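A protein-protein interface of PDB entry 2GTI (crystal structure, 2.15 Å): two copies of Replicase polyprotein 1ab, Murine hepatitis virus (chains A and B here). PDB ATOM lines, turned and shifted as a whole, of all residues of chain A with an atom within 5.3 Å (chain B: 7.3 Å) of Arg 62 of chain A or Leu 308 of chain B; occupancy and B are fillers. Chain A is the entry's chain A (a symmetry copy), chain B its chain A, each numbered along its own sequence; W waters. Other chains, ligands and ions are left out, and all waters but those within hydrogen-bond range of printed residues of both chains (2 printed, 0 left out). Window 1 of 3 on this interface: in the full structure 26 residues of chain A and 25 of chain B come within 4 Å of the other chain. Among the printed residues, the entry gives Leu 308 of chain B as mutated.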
ATOM      1  N   LEU A  10      32.342  19.240  -4.712  1.00  0.00           N
ATOM      2  CA  LEU A  10      31.751  17.938  -4.424  1.00  0.00           C
ATOM      3  C   LEU A  10      32.829  16.916  -4.071  1.00  0.00           C
ATOM      4  O   LEU A  10      32.694  16.173  -3.104  1.00  0.00           O
ATOM      5  CB  LEU A  10      30.931  17.444  -5.623  1.00  0.00           C
ATOM      6  CG  LEU A  10      30.000  16.263  -5.338  1.00  0.00           C
ATOM      7  CD1 LEU A  10      28.942  16.702  -4.340  1.00  0.00           C
ATOM      8  CD2 LEU A  10      29.341  15.770  -6.634  1.00  0.00           C
ATOM      9  N   GLY A  14      32.429  17.231  -0.288  1.00  0.00           N
ATOM     10  CA  GLY A  14      31.217  16.440  -0.211  1.00  0.00           C
ATOM     11  C   GLY A  14      29.989  17.255  -0.573  1.00  0.00           C
ATOM     12  O   GLY A  14      28.916  16.695  -0.813  1.00  0.00           O
ATOM     13  N   HIS A  15      30.146  18.577  -0.601  1.00  0.00           N
ATOM     14  CA  HIS A  15      29.059  19.490  -0.963  1.00  0.00           C
ATOM     15  C   HIS A  15      29.658  20.854  -1.285  1.00  0.00           C
ATOM     16  O   HIS A  15      30.850  21.075  -1.085  1.00  0.00           O
ATOM     17  CB  HIS A  15      28.049  19.617   0.182  1.00  0.00           C
ATOM     18  CG  HIS A  15      28.611  20.267   1.402  1.00  0.00           C
ATOM     19  ND1 HIS A  15      28.163  21.485   1.869  1.00  0.00           N
ATOM     20  CD2 HIS A  15      29.625  19.898   2.219  1.00  0.00           C
ATOM     21  CE1 HIS A  15      28.882  21.840   2.919  1.00  0.00           C
ATOM     22  NE2 HIS A  15      29.775  20.894   3.152  1.00  0.00           N
ATOM     23  N   GLU A  57      25.056  20.275  -9.762  1.00  0.00           N
ATOM     24  CA  GLU A  57      25.192  21.524  -9.023  1.00  0.00           C
ATOM     25  C   GLU A  57      24.163  21.551  -7.897  1.00  0.00           C
ATOM     26  O   GLU A  57      24.462  21.975  -6.784  1.00  0.00           O
ATOM     27  CB  GLU A  57      24.954  22.747  -9.917  1.00  0.00           C
ATOM     28  CG  GLU A  57      25.098  24.062  -9.141  1.00  0.00           C
ATOM     29  CD  GLU A  57      24.636  25.275  -9.922  1.00  0.00           C
ATOM     30  OE1 GLU A  57      24.790  25.278 -11.158  1.00  0.00           O
ATOM     31  OE2 GLU A  57      24.131  26.239  -9.295  1.00  0.00           O
ATOM     32  N   LEU A  58      22.947  21.100  -8.205  1.00  0.00           N
ATOM     33  CA  LEU A  58      21.861  21.073  -7.225  1.00  0.00           C
ATOM     34  C   LEU A  58      22.136  20.066  -6.120  1.00  0.00           C
ATOM     35  O   LEU A  58      21.811  20.306  -4.959  1.00  0.00           O
ATOM     36  CB  LEU A  58      20.537  20.728  -7.904  1.00  0.00           C
ATOM     37  CG  LEU A  58      19.917  21.804  -8.802  1.00  0.00           C
ATOM     38  CD1 LEU A  58      18.705  21.220  -9.495  1.00  0.00           C
ATOM     39  CD2 LEU A  58      19.515  23.015  -7.968  1.00  0.00           C
ATOM     40  N   PHE A  59      22.715  18.929  -6.481  1.00  0.00           N
ATOM     41  CA  PHE A  59      23.029  17.920  -5.481  1.00  0.00           C
ATOM     42  C   PHE A  59      24.138  18.462  -4.570  1.00  0.00           C
ATOM     43  O   PHE A  59      24.065  18.350  -3.349  1.00  0.00           O
ATOM     44  CB  PHE A  59      23.477  16.616  -6.155  1.00  0.00           C
ATOM     45  CG  PHE A  59      24.055  15.603  -5.195  1.00  0.00           C
ATOM     46  CD1 PHE A  59      23.241  14.944  -4.286  1.00  0.00           C
ATOM     47  CD2 PHE A  59      25.422  15.341  -5.188  1.00  0.00           C
ATOM     48  CE1 PHE A  59      23.777  14.031  -3.372  1.00  0.00           C
ATOM     49  CE2 PHE A  59      25.974  14.433  -4.283  1.00  0.00           C
ATOM     50  CZ  PHE A  59      25.150  13.774  -3.369  1.00  0.00           C
ATOM     51  N   ALA A  60      25.161  19.061  -5.171  1.00  0.00           N
ATOM     52  CA  ALA A  60      26.270  19.607  -4.393  1.00  0.00           C
ATOM     53  C   ALA A  60      25.789  20.689  -3.432  1.00  0.00           C
ATOM     54  O   ALA A  60      26.352  20.857  -2.355  1.00  0.00           O
ATOM     55  CB  ALA A  60      27.333  20.175  -5.324  1.00  0.00           C
ATOM     56  N   LYS A  61      24.743  21.414  -3.816  1.00  0.00           N
ATOM     57  CA  LYS A  61      24.228  22.482  -2.970  1.00  0.00           C
ATOM     58  C   LYS A  61      23.149  22.015  -2.007  1.00  0.00           C
ATOM     59  O   LYS A  61      22.566  22.812  -1.285  1.00  0.00           O
ATOM     60  CB  LYS A  61      23.703  23.630  -3.839  1.00  0.00           C
ATOM     61  CG  LYS A  61      24.804  24.438  -4.497  1.00  0.00           C
ATOM     62  CD  LYS A  61      24.252  25.549  -5.376  1.00  0.00           C
ATOM     63  CE  LYS A  61      25.376  26.413  -5.937  1.00  0.00           C
ATOM     64  NZ  LYS A  61      24.882  27.354  -6.973  1.00  0.00           N
ATOM     65  N   ARG A  62      22.889  20.714  -1.998  1.00  0.00           N
ATOM     66  CA  ARG A  62      21.875  20.149  -1.128  1.00  0.00           C
ATOM     67  C   ARG A  62      22.129  20.497   0.335  1.00  0.00           C
ATOM     68  O   ARG A  62      23.270  20.705   0.765  1.00  0.00           O
ATOM     69  CB  ARG A  62      21.845  18.628  -1.269  1.00  0.00           C
ATOM     70  CG  ARG A  62      23.058  17.940  -0.663  1.00  0.00           C
ATOM     71  CD  ARG A  62      23.140  16.464  -1.054  1.00  0.00           C
ATOM     72  NE  ARG A  62      24.234  15.789  -0.355  1.00  0.00           N
ATOM     73  CZ  ARG A  62      25.530  16.037  -0.544  1.00  0.00           C
ATOM     74  NH1 ARG A  62      25.928  16.948  -1.423  1.00  0.00           N
ATOM     75  NH2 ARG A  62      26.429  15.383   0.171  1.00  0.00           N
ATOM     76  N   SER A  63      21.048  20.549   1.097  1.00  0.00           N
ATOM     77  CA  SER A  63      21.143  20.833   2.515  1.00  0.00           C
ATOM     78  C   SER A  63      21.759  19.637   3.226  1.00  0.00           C
ATOM     79  O   SER A  63      21.336  18.504   3.012  1.00  0.00           O
ATOM     80  CB  SER A  63      19.750  21.101   3.080  1.00  0.00           C
ATOM     81  OG  SER A  63      19.304  22.406   2.775  1.00  0.00           O
ATOM     82  N   ILE A  64      22.769  19.875   4.054  1.00  0.00           N
ATOM     83  CA  ILE A  64      23.382  18.772   4.792  1.00  0.00           C
ATOM     84  C   ILE A  64      23.118  18.911   6.287  1.00  0.00           C
ATOM     85  O   ILE A  64      23.755  18.258   7.113  1.00  0.00           O
ATOM     86  CB  ILE A  64      24.916  18.650   4.506  1.00  0.00           C
ATOM     87  CG1 ILE A  64      25.604  20.010   4.591  1.00  0.00           C
ATOM     88  CG2 ILE A  64      25.135  18.076   3.110  1.00  0.00           C
ATOM     89  CD1 ILE A  64      26.244  20.286   5.898  1.00  0.00           C
ATOM     90  N   VAL A  85      18.233  24.160  -1.032  1.00  0.00           N
ATOM     91  CA  VAL A  85      17.646  23.064  -1.783  1.00  0.00           C
ATOM     92  C   VAL A  85      17.632  21.807  -0.928  1.00  0.00           C
ATOM     93  O   VAL A  85      18.594  21.509  -0.213  1.00  0.00           O
ATOM     94  CB  VAL A  85      18.411  22.816  -3.104  1.00  0.00           C
ATOM     95  CG1 VAL A  85      19.869  22.509  -2.816  1.00  0.00           C
ATOM     96  CG2 VAL A  85      17.759  21.694  -3.876  1.00  0.00           C
ATOM     97  N   TRP A  87      17.393  17.743  -0.771  1.00  0.00           N
ATOM     98  CA  TRP A  87      17.588  16.544  -1.556  1.00  0.00           C
ATOM     99  C   TRP A  87      16.749  15.425  -0.966  1.00  0.00           C
ATOM    100  O   TRP A  87      16.793  15.160   0.239  1.00  0.00           O
ATOM    101  CB  TRP A  87      19.061  16.131  -1.570  1.00  0.00           C
ATOM    102  CG  TRP A  87      19.323  15.026  -2.529  1.00  0.00           C
ATOM    103  CD1 TRP A  87      19.397  13.695  -2.245  1.00  0.00           C
ATOM    104  CD2 TRP A  87      19.522  15.150  -3.942  1.00  0.00           C
ATOM    105  NE1 TRP A  87      19.637  12.981  -3.390  1.00  0.00           N
ATOM    106  CE2 TRP A  87      19.717  13.848  -4.449  1.00  0.00           C
ATOM    107  CE3 TRP A  87      19.558  16.239  -4.833  1.00  0.00           C
ATOM    108  CZ2 TRP A  87      19.943  13.597  -5.808  1.00  0.00           C
ATOM    109  CZ3 TRP A  87      19.785  15.991  -6.186  1.00  0.00           C
ATOM    110  CH2 TRP A  87      19.975  14.678  -6.660  1.00  0.00           C
ATOM    111  N   TYR A  89      16.474  11.765  -0.781  1.00  0.00           N
ATOM    112  CA  TYR A  89      17.247  10.547  -0.967  1.00  0.00           C
ATOM    113  C   TYR A  89      16.444   9.311  -1.343  1.00  0.00           C
ATOM    114  O   TYR A  89      16.995   8.361  -1.896  1.00  0.00           O
ATOM    115  CB  TYR A  89      18.064  10.270   0.293  1.00  0.00           C
ATOM    116  CG  TYR A  89      19.205  11.246   0.481  1.00  0.00           C
ATOM    117  CD1 TYR A  89      20.428  11.034  -0.140  1.00  0.00           C
ATOM    118  CD2 TYR A  89      19.054  12.384   1.274  1.00  0.00           C
ATOM    119  CE1 TYR A  89      21.479  11.919   0.018  1.00  0.00           C
ATOM    120  CE2 TYR A  89      20.109  13.287   1.445  1.00  0.00           C
ATOM    121  CZ  TYR A  89      21.319  13.041   0.810  1.00  0.00           C
ATOM    122  OH  TYR A  89      22.372  13.907   0.959  1.00  0.00           O
ATOM    123  N   ASN A 158      20.682  13.951   5.876  1.00  0.00           N
ATOM    124  CA  ASN A 158      21.394  13.287   4.797  1.00  0.00           C
ATOM    125  C   ASN A 158      20.653  12.005   4.409  1.00  0.00           C
ATOM    126  O   ASN A 158      21.269  10.988   4.079  1.00  0.00           O
ATOM    127  CB  ASN A 158      22.823  12.979   5.237  1.00  0.00           C
ATOM    128  CG  ASN A 158      23.572  14.225   5.673  1.00  0.00           C
ATOM    129  OD1 ASN A 158      24.224  14.238   6.723  1.00  0.00           O
ATOM    130  ND2 ASN A 158      23.486  15.283   4.870  1.00  0.00           N
ATOM    131  N   ILE B 274      30.481  14.865  14.424  1.00  0.00           N
ATOM    132  CA  ILE B 274      31.151  13.694  14.962  1.00  0.00           C
ATOM    133  C   ILE B 274      32.594  14.061  15.282  1.00  0.00           C
ATOM    134  O   ILE B 274      33.195  14.895  14.610  1.00  0.00           O
ATOM    135  CB  ILE B 274      31.133  12.537  13.941  1.00  0.00           C
ATOM    136  CG1 ILE B 274      29.684  12.106  13.677  1.00  0.00           C
ATOM    137  CG2 ILE B 274      31.964  11.367  14.459  1.00  0.00           C
ATOM    138  CD1 ILE B 274      29.542  11.048  12.609  1.00  0.00           C
ATOM    139  N   VAL B 293      25.587   5.619   8.271  1.00  0.00           N
ATOM    140  CA  VAL B 293      25.362   5.733   6.841  1.00  0.00           C
ATOM    141  C   VAL B 293      26.521   6.516   6.247  1.00  0.00           C
ATOM    142  O   VAL B 293      26.847   7.614   6.705  1.00  0.00           O
ATOM    143  CB  VAL B 293      24.015   6.424   6.553  1.00  0.00           C
ATOM    144  CG1 VAL B 293      23.812   6.588   5.061  1.00  0.00           C
ATOM    145  CG2 VAL B 293      22.878   5.589   7.152  1.00  0.00           C
ATOM    146  N   ILE B 294      27.152   5.929   5.238  1.00  0.00           N
ATOM    147  CA  ILE B 294      28.299   6.533   4.584  1.00  0.00           C
ATOM    148  C   ILE B 294      28.023   6.975   3.150  1.00  0.00           C
ATOM    149  O   ILE B 294      27.428   6.237   2.362  1.00  0.00           O
ATOM    150  CB  ILE B 294      29.482   5.542   4.514  1.00  0.00           C
ATOM    151  CG1 ILE B 294      29.772   4.940   5.889  1.00  0.00           C
ATOM    152  CG2 ILE B 294      30.703   6.242   3.961  1.00  0.00           C
ATOM    153  CD1 ILE B 294      30.335   5.912   6.898  1.00  0.00           C
ATOM    154  N   GLN B 295      28.450   8.188   2.823  1.00  0.00           N
ATOM    155  CA  GLN B 295      28.328   8.701   1.464  1.00  0.00           C
ATOM    156  C   GLN B 295      29.756   8.938   0.986  1.00  0.00           C
ATOM    157  O   GLN B 295      30.552   9.555   1.689  1.00  0.00           O
ATOM    158  CB  GLN B 295      27.560  10.024   1.425  1.00  0.00           C
ATOM    159  CG  GLN B 295      26.081   9.903   1.734  1.00  0.00           C
ATOM    160  CD  GLN B 295      25.372  11.240   1.674  1.00  0.00           C
ATOM    161  OE1 GLN B 295      25.193  11.819   0.601  1.00  0.00           O
ATOM    162  NE2 GLN B 295      24.978  11.746   2.832  1.00  0.00           N
ATOM    163  N   GLU B 296      30.084   8.428  -0.194  1.00  0.00           N
ATOM    164  CA  GLU B 296      31.415   8.617  -0.753  1.00  0.00           C
ATOM    165  C   GLU B 296      31.288   9.219  -2.150  1.00  0.00           C
ATOM    166  O   GLU B 296      30.569   8.697  -3.005  1.00  0.00           O
ATOM    167  CB  GLU B 296      32.177   7.290  -0.809  1.00  0.00           C
ATOM    168  CG  GLU B 296      33.579   7.435  -1.370  1.00  0.00           C
ATOM    169  CD  GLU B 296      34.475   6.266  -1.035  1.00  0.00           C
ATOM    170  OE1 GLU B 296      34.034   5.106  -1.189  1.00  0.00           O
ATOM    171  OE2 GLU B 296      35.628   6.512  -0.626  1.00  0.00           O
ATOM    172  N   PHE B 297      32.008  10.311  -2.377  1.00  0.00           N
ATOM    173  CA  PHE B 297      31.945  11.026  -3.644  1.00  0.00           C
ATOM    174  C   PHE B 297      32.911  10.555  -4.734  1.00  0.00           C
ATOM    175  O   PHE B 297      32.576  10.589  -5.920  1.00  0.00           O
ATOM    176  CB  PHE B 297      32.082  12.508  -3.327  1.00  0.00           C
ATOM    177  CG  PHE B 297      31.115  12.959  -2.266  1.00  0.00           C
ATOM    178  CD1 PHE B 297      29.785  13.225  -2.584  1.00  0.00           C
ATOM    179  CD2 PHE B 297      31.503  12.996  -0.924  1.00  0.00           C
ATOM    180  CE1 PHE B 297      28.851  13.518  -1.589  1.00  0.00           C
ATOM    181  CE2 PHE B 297      30.574  13.286   0.082  1.00  0.00           C
ATOM    182  CZ  PHE B 297      29.247  13.546  -0.255  1.00  0.00           C
ATOM    183  N   SER B 306      37.512   9.326   2.153  1.00  0.00           N
ATOM    184  CA  SER B 306      36.933  10.568   2.645  1.00  0.00           C
ATOM    185  C   SER B 306      35.415  10.422   2.578  1.00  0.00           C
ATOM    186  O   SER B 306      34.834  10.386   1.496  1.00  0.00           O
ATOM    187  CB  SER B 306      37.399  11.742   1.788  1.00  0.00           C
ATOM    188  OG  SER B 306      36.974  12.965   2.354  1.00  0.00           O
ATOM    189  N   TYR B 307      34.776  10.338   3.741  1.00  0.00           N
ATOM    190  CA  TYR B 307      33.334  10.148   3.792  1.00  0.00           C
ATOM    191  C   TYR B 307      32.523  11.272   4.413  1.00  0.00           C
ATOM    192  O   TYR B 307      33.035  12.101   5.171  1.00  0.00           O
ATOM    193  CB  TYR B 307      32.985   8.888   4.596  1.00  0.00           C
ATOM    194  CG  TYR B 307      33.631   7.591   4.161  1.00  0.00           C
ATOM    195  CD1 TYR B 307      33.625   7.194   2.828  1.00  0.00           C
ATOM    196  CD2 TYR B 307      34.168   6.718   5.104  1.00  0.00           C
ATOM    197  CE1 TYR B 307      34.131   5.956   2.446  1.00  0.00           C
ATOM    198  CE2 TYR B 307      34.675   5.474   4.735  1.00  0.00           C
ATOM    199  CZ  TYR B 307      34.649   5.098   3.409  1.00  0.00           C
ATOM    200  OH  TYR B 307      35.106   3.855   3.049  1.00  0.00           O
ATOM    201  N   LEU B 308      31.239  11.276   4.075  1.00  0.00           N
ATOM    202  CA  LEU B 308      30.277  12.192   4.671  1.00  0.00           C
ATOM    203  C   LEU B 308      29.570  11.149   5.528  1.00  0.00           C
ATOM    204  O   LEU B 308      28.875  10.290   4.998  1.00  0.00           O
ATOM    205  CB  LEU B 308      29.310  12.767   3.632  1.00  0.00           C
ATOM    206  CG  LEU B 308      28.037  13.386   4.228  1.00  0.00           C
ATOM    207  CD1 LEU B 308      28.387  14.307   5.378  1.00  0.00           C
ATOM    208  CD2 LEU B 308      27.274  14.137   3.159  1.00  0.00           C
ATOM    209  N   ILE B 309      29.772  11.204   6.837  1.00  0.00           N
ATOM    210  CA  ILE B 309      29.201  10.216   7.756  1.00  0.00           C
ATOM    211  C   ILE B 309      28.060  10.721   8.637  1.00  0.00           C
ATOM    212  O   ILE B 309      28.145  11.804   9.213  1.00  0.00           O
ATOM    213  CB  ILE B 309      30.304   9.663   8.698  1.00  0.00           C
ATOM    214  CG1 ILE B 309      31.458   9.107   7.863  1.00  0.00           C
ATOM    215  CG2 ILE B 309      29.725   8.597   9.623  1.00  0.00           C
ATOM    216  CD1 ILE B 309      32.652   8.636   8.682  1.00  0.00           C
ATOM    217  N   THR B 310      27.014   9.910   8.754  1.00  0.00           N
ATOM    218  CA  THR B 310      25.853  10.227   9.578  1.00  0.00           C
ATOM    219  C   THR B 310      25.555   9.067  10.535  1.00  0.00           C
ATOM    220  O   THR B 310      25.341   7.936  10.094  1.00  0.00           O
ATOM    221  CB  THR B 310      24.596  10.467   8.705  1.00  0.00           C
ATOM    222  OG1 THR B 310      24.849  11.531   7.775  1.00  0.00           O
ATOM    223  CG2 THR B 310      23.401  10.855   9.585  1.00  0.00           C
ATOM    224  N   SER B 317      26.939  14.014  12.730  1.00  0.00           N
ATOM    225  CA  SER B 317      27.513  13.801  11.401  1.00  0.00           C
ATOM    226  C   SER B 317      28.743  14.681  11.123  1.00  0.00           C
ATOM    227  O   SER B 317      28.991  15.657  11.833  1.00  0.00           O
ATOM    228  CB  SER B 317      26.446  14.048  10.324  1.00  0.00           C
ATOM    229  OG  SER B 317      26.058  15.413  10.269  1.00  0.00           O
ATOM    230  N   LYS B 318      29.519  14.311  10.102  1.00  0.00           N
ATOM    231  CA  LYS B 318      30.708  15.067   9.703  1.00  0.00           C
ATOM    232  C   LYS B 318      30.820  15.012   8.180  1.00  0.00           C
ATOM    233  O   LYS B 318      30.630  13.953   7.579  1.00  0.00           O
ATOM    234  CB  LYS B 318      31.980  14.489  10.339  1.00  0.00           C
ATOM    235  CG  LYS B 318      33.154  15.475  10.327  1.00  0.00           C
ATOM    236  CD  LYS B 318      34.485  14.845  10.737  1.00  0.00           C
ATOM    237  CE  LYS B 318      34.425  14.250  12.125  1.00  0.00           C
ATOM    238  NZ  LYS B 318      35.759  13.795  12.622  1.00  0.00           N
ATOM    239  N   SER B 319      31.139  16.142   7.559  1.00  0.00           N
ATOM    240  CA  SER B 319      31.226  16.218   6.100  1.00  0.00           C
ATOM    241  C   SER B 319      32.419  15.529   5.444  1.00  0.00           C
ATOM    242  O   SER B 319      32.259  14.809   4.455  1.00  0.00           O
ATOM    243  CB  SER B 319      31.195  17.678   5.657  1.00  0.00           C
ATOM    244  OG  SER B 319      29.975  18.283   6.035  1.00  0.00           O
ATOM    245  N   VAL B 320      33.612  15.764   5.972  1.00  0.00           N
ATOM    246  CA  VAL B 320      34.810  15.159   5.410  1.00  0.00           C
ATOM    247  C   VAL B 320      35.558  14.384   6.483  1.00  0.00           C
ATOM    248  O   VAL B 320      36.514  14.876   7.079  1.00  0.00           O
ATOM    249  CB  VAL B 320      35.734  16.235   4.797  1.00  0.00           C
ATOM    250  CG1 VAL B 320      36.991  15.587   4.221  1.00  0.00           C
ATOM    251  CG2 VAL B 320      34.989  16.989   3.710  1.00  0.00           C
ATOM    252  N   CYS B 321      35.105  13.164   6.729  1.00  0.00           N
ATOM    253  CA  CYS B 321      35.720  12.315   7.734  1.00  0.00           C
ATOM    254  C   CYS B 321      36.660  11.310   7.075  1.00  0.00           C
ATOM    255  O   CYS B 321      36.220  10.341   6.452  1.00  0.00           O
ATOM    256  CB  CYS B 321      34.635  11.579   8.524  1.00  0.00           C
ATOM    257  SG  CYS B 321      35.267  10.608   9.895  1.00  0.00           S
HETATM  258  O   HOH W   1      25.557  16.339   7.687  1.00  0.00           O
HETATM  259  O   HOH W   2      23.632   9.879   3.928  1.00  0.00           O
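The side-chain amide oxygen (OD1) of Asn 158 of chain A is in hydrogen-bond range of the side-chain hydroxyl (OG1) of Thr 310 of chain B (3.0 Å).
O of Gln 295 of chain B lies within hydrogen-bond range of N of Leu 308 of chain B (3.0 Å).
N of Val 293 of chain B sits at hydrogen-bond distance from O of Thr 310 of chain B, 3.0 Å away.
The guanidinium group of Arg 62 of chain A is in hydrogen-bond range of the backbone carbonyl oxygen of Gly 14 of chain A (3.0 Å).
The backbone carbonyl oxygen of Phe 59 of chain A sits close to the guanidinium group of Arg 62 of chain A.
The guanidinium group (NE) of Arg 62 of chain A lies within hydrogen-bond range of the side-chain hydroxyl (OH) of Tyr 89 of chain A (3.0 Å).
Among the printed residues, pairs that only touch across the chains: Leu 10 of chain A with Phe 297 of chain B (3.7 Å), Gly 14 of chain A with Phe 297 of chain B (3.2 Å), His 15 of chain A with Ser 319 of chain B (3.9 Å), Arg 62 of chain A with Gln 295 of chain B (3.8 Å), Arg 62 of chain A with Phe 297 of chain B (3.4 Å), Arg 62 of chain A with Leu 308 of chain B (3.3 Å), Tyr 89 of chain A with Gln 295 of chain B (3.5 Å) and Asn 158 of chain A with Gln 295 of chain B (3.5 Å).
Leu 308 of chain B touches just one residue of chain A: Arg 62 (3.3 Å).
Of the printed residues of chain B, Tyr 89 of chain A touches Gln 295.
Of the printed residues of chain A, Thr 310 of chain B touches Asn 158.
Ser 63 of chain A touches none of the printed residues of chain B.
Ala 60 of chain A touches none of the printed residues of chain B.
The nearest printed residue of chain B that does not touch Arg 62 of chain A is Ser 319 of chain B (7.3 Å).
The nearest printed residue of chain A that does not touch Gln 295 of chain B is Phe 59 of chain A (4.4 Å).
Of the 15 printed residues of chain A, 6 touch a printed residue of chain B.
Printed residues of chain A that touch a printed residue of chain B: Leu 10, Gly 14, His 15, Arg 62, Tyr 89 and Asn 158.
Hydrophobic or aromatic side chains of chain A within 4 Å of the printed part of chain B: Leu 10, His 15 and Tyr 89.
Among the printed residues, no Asp or Glu carboxylate lies within 4 Å of a Lys or Arg side-chain nitrogen of the other chain.
No position is printed for both chains.
Of the 9 pairs that touch across the chains among the printed residues, none has its exchanged pair printed and touching as well.
Water W2 lies within hydrogen-bond range of NE2 of Gln 295 of chain B (2.5 Å) and O of Asn 158 of chain A (2.6 Å).
Water W1 lies within hydrogen-bond range of the side-chain amide oxygen (OD1) of Asn 158 of chain A, the backbone carbonyl oxygen (O) of Ile 64 of chain A and the side-chain hydroxyl (OG) of Ser 317 of chain B.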
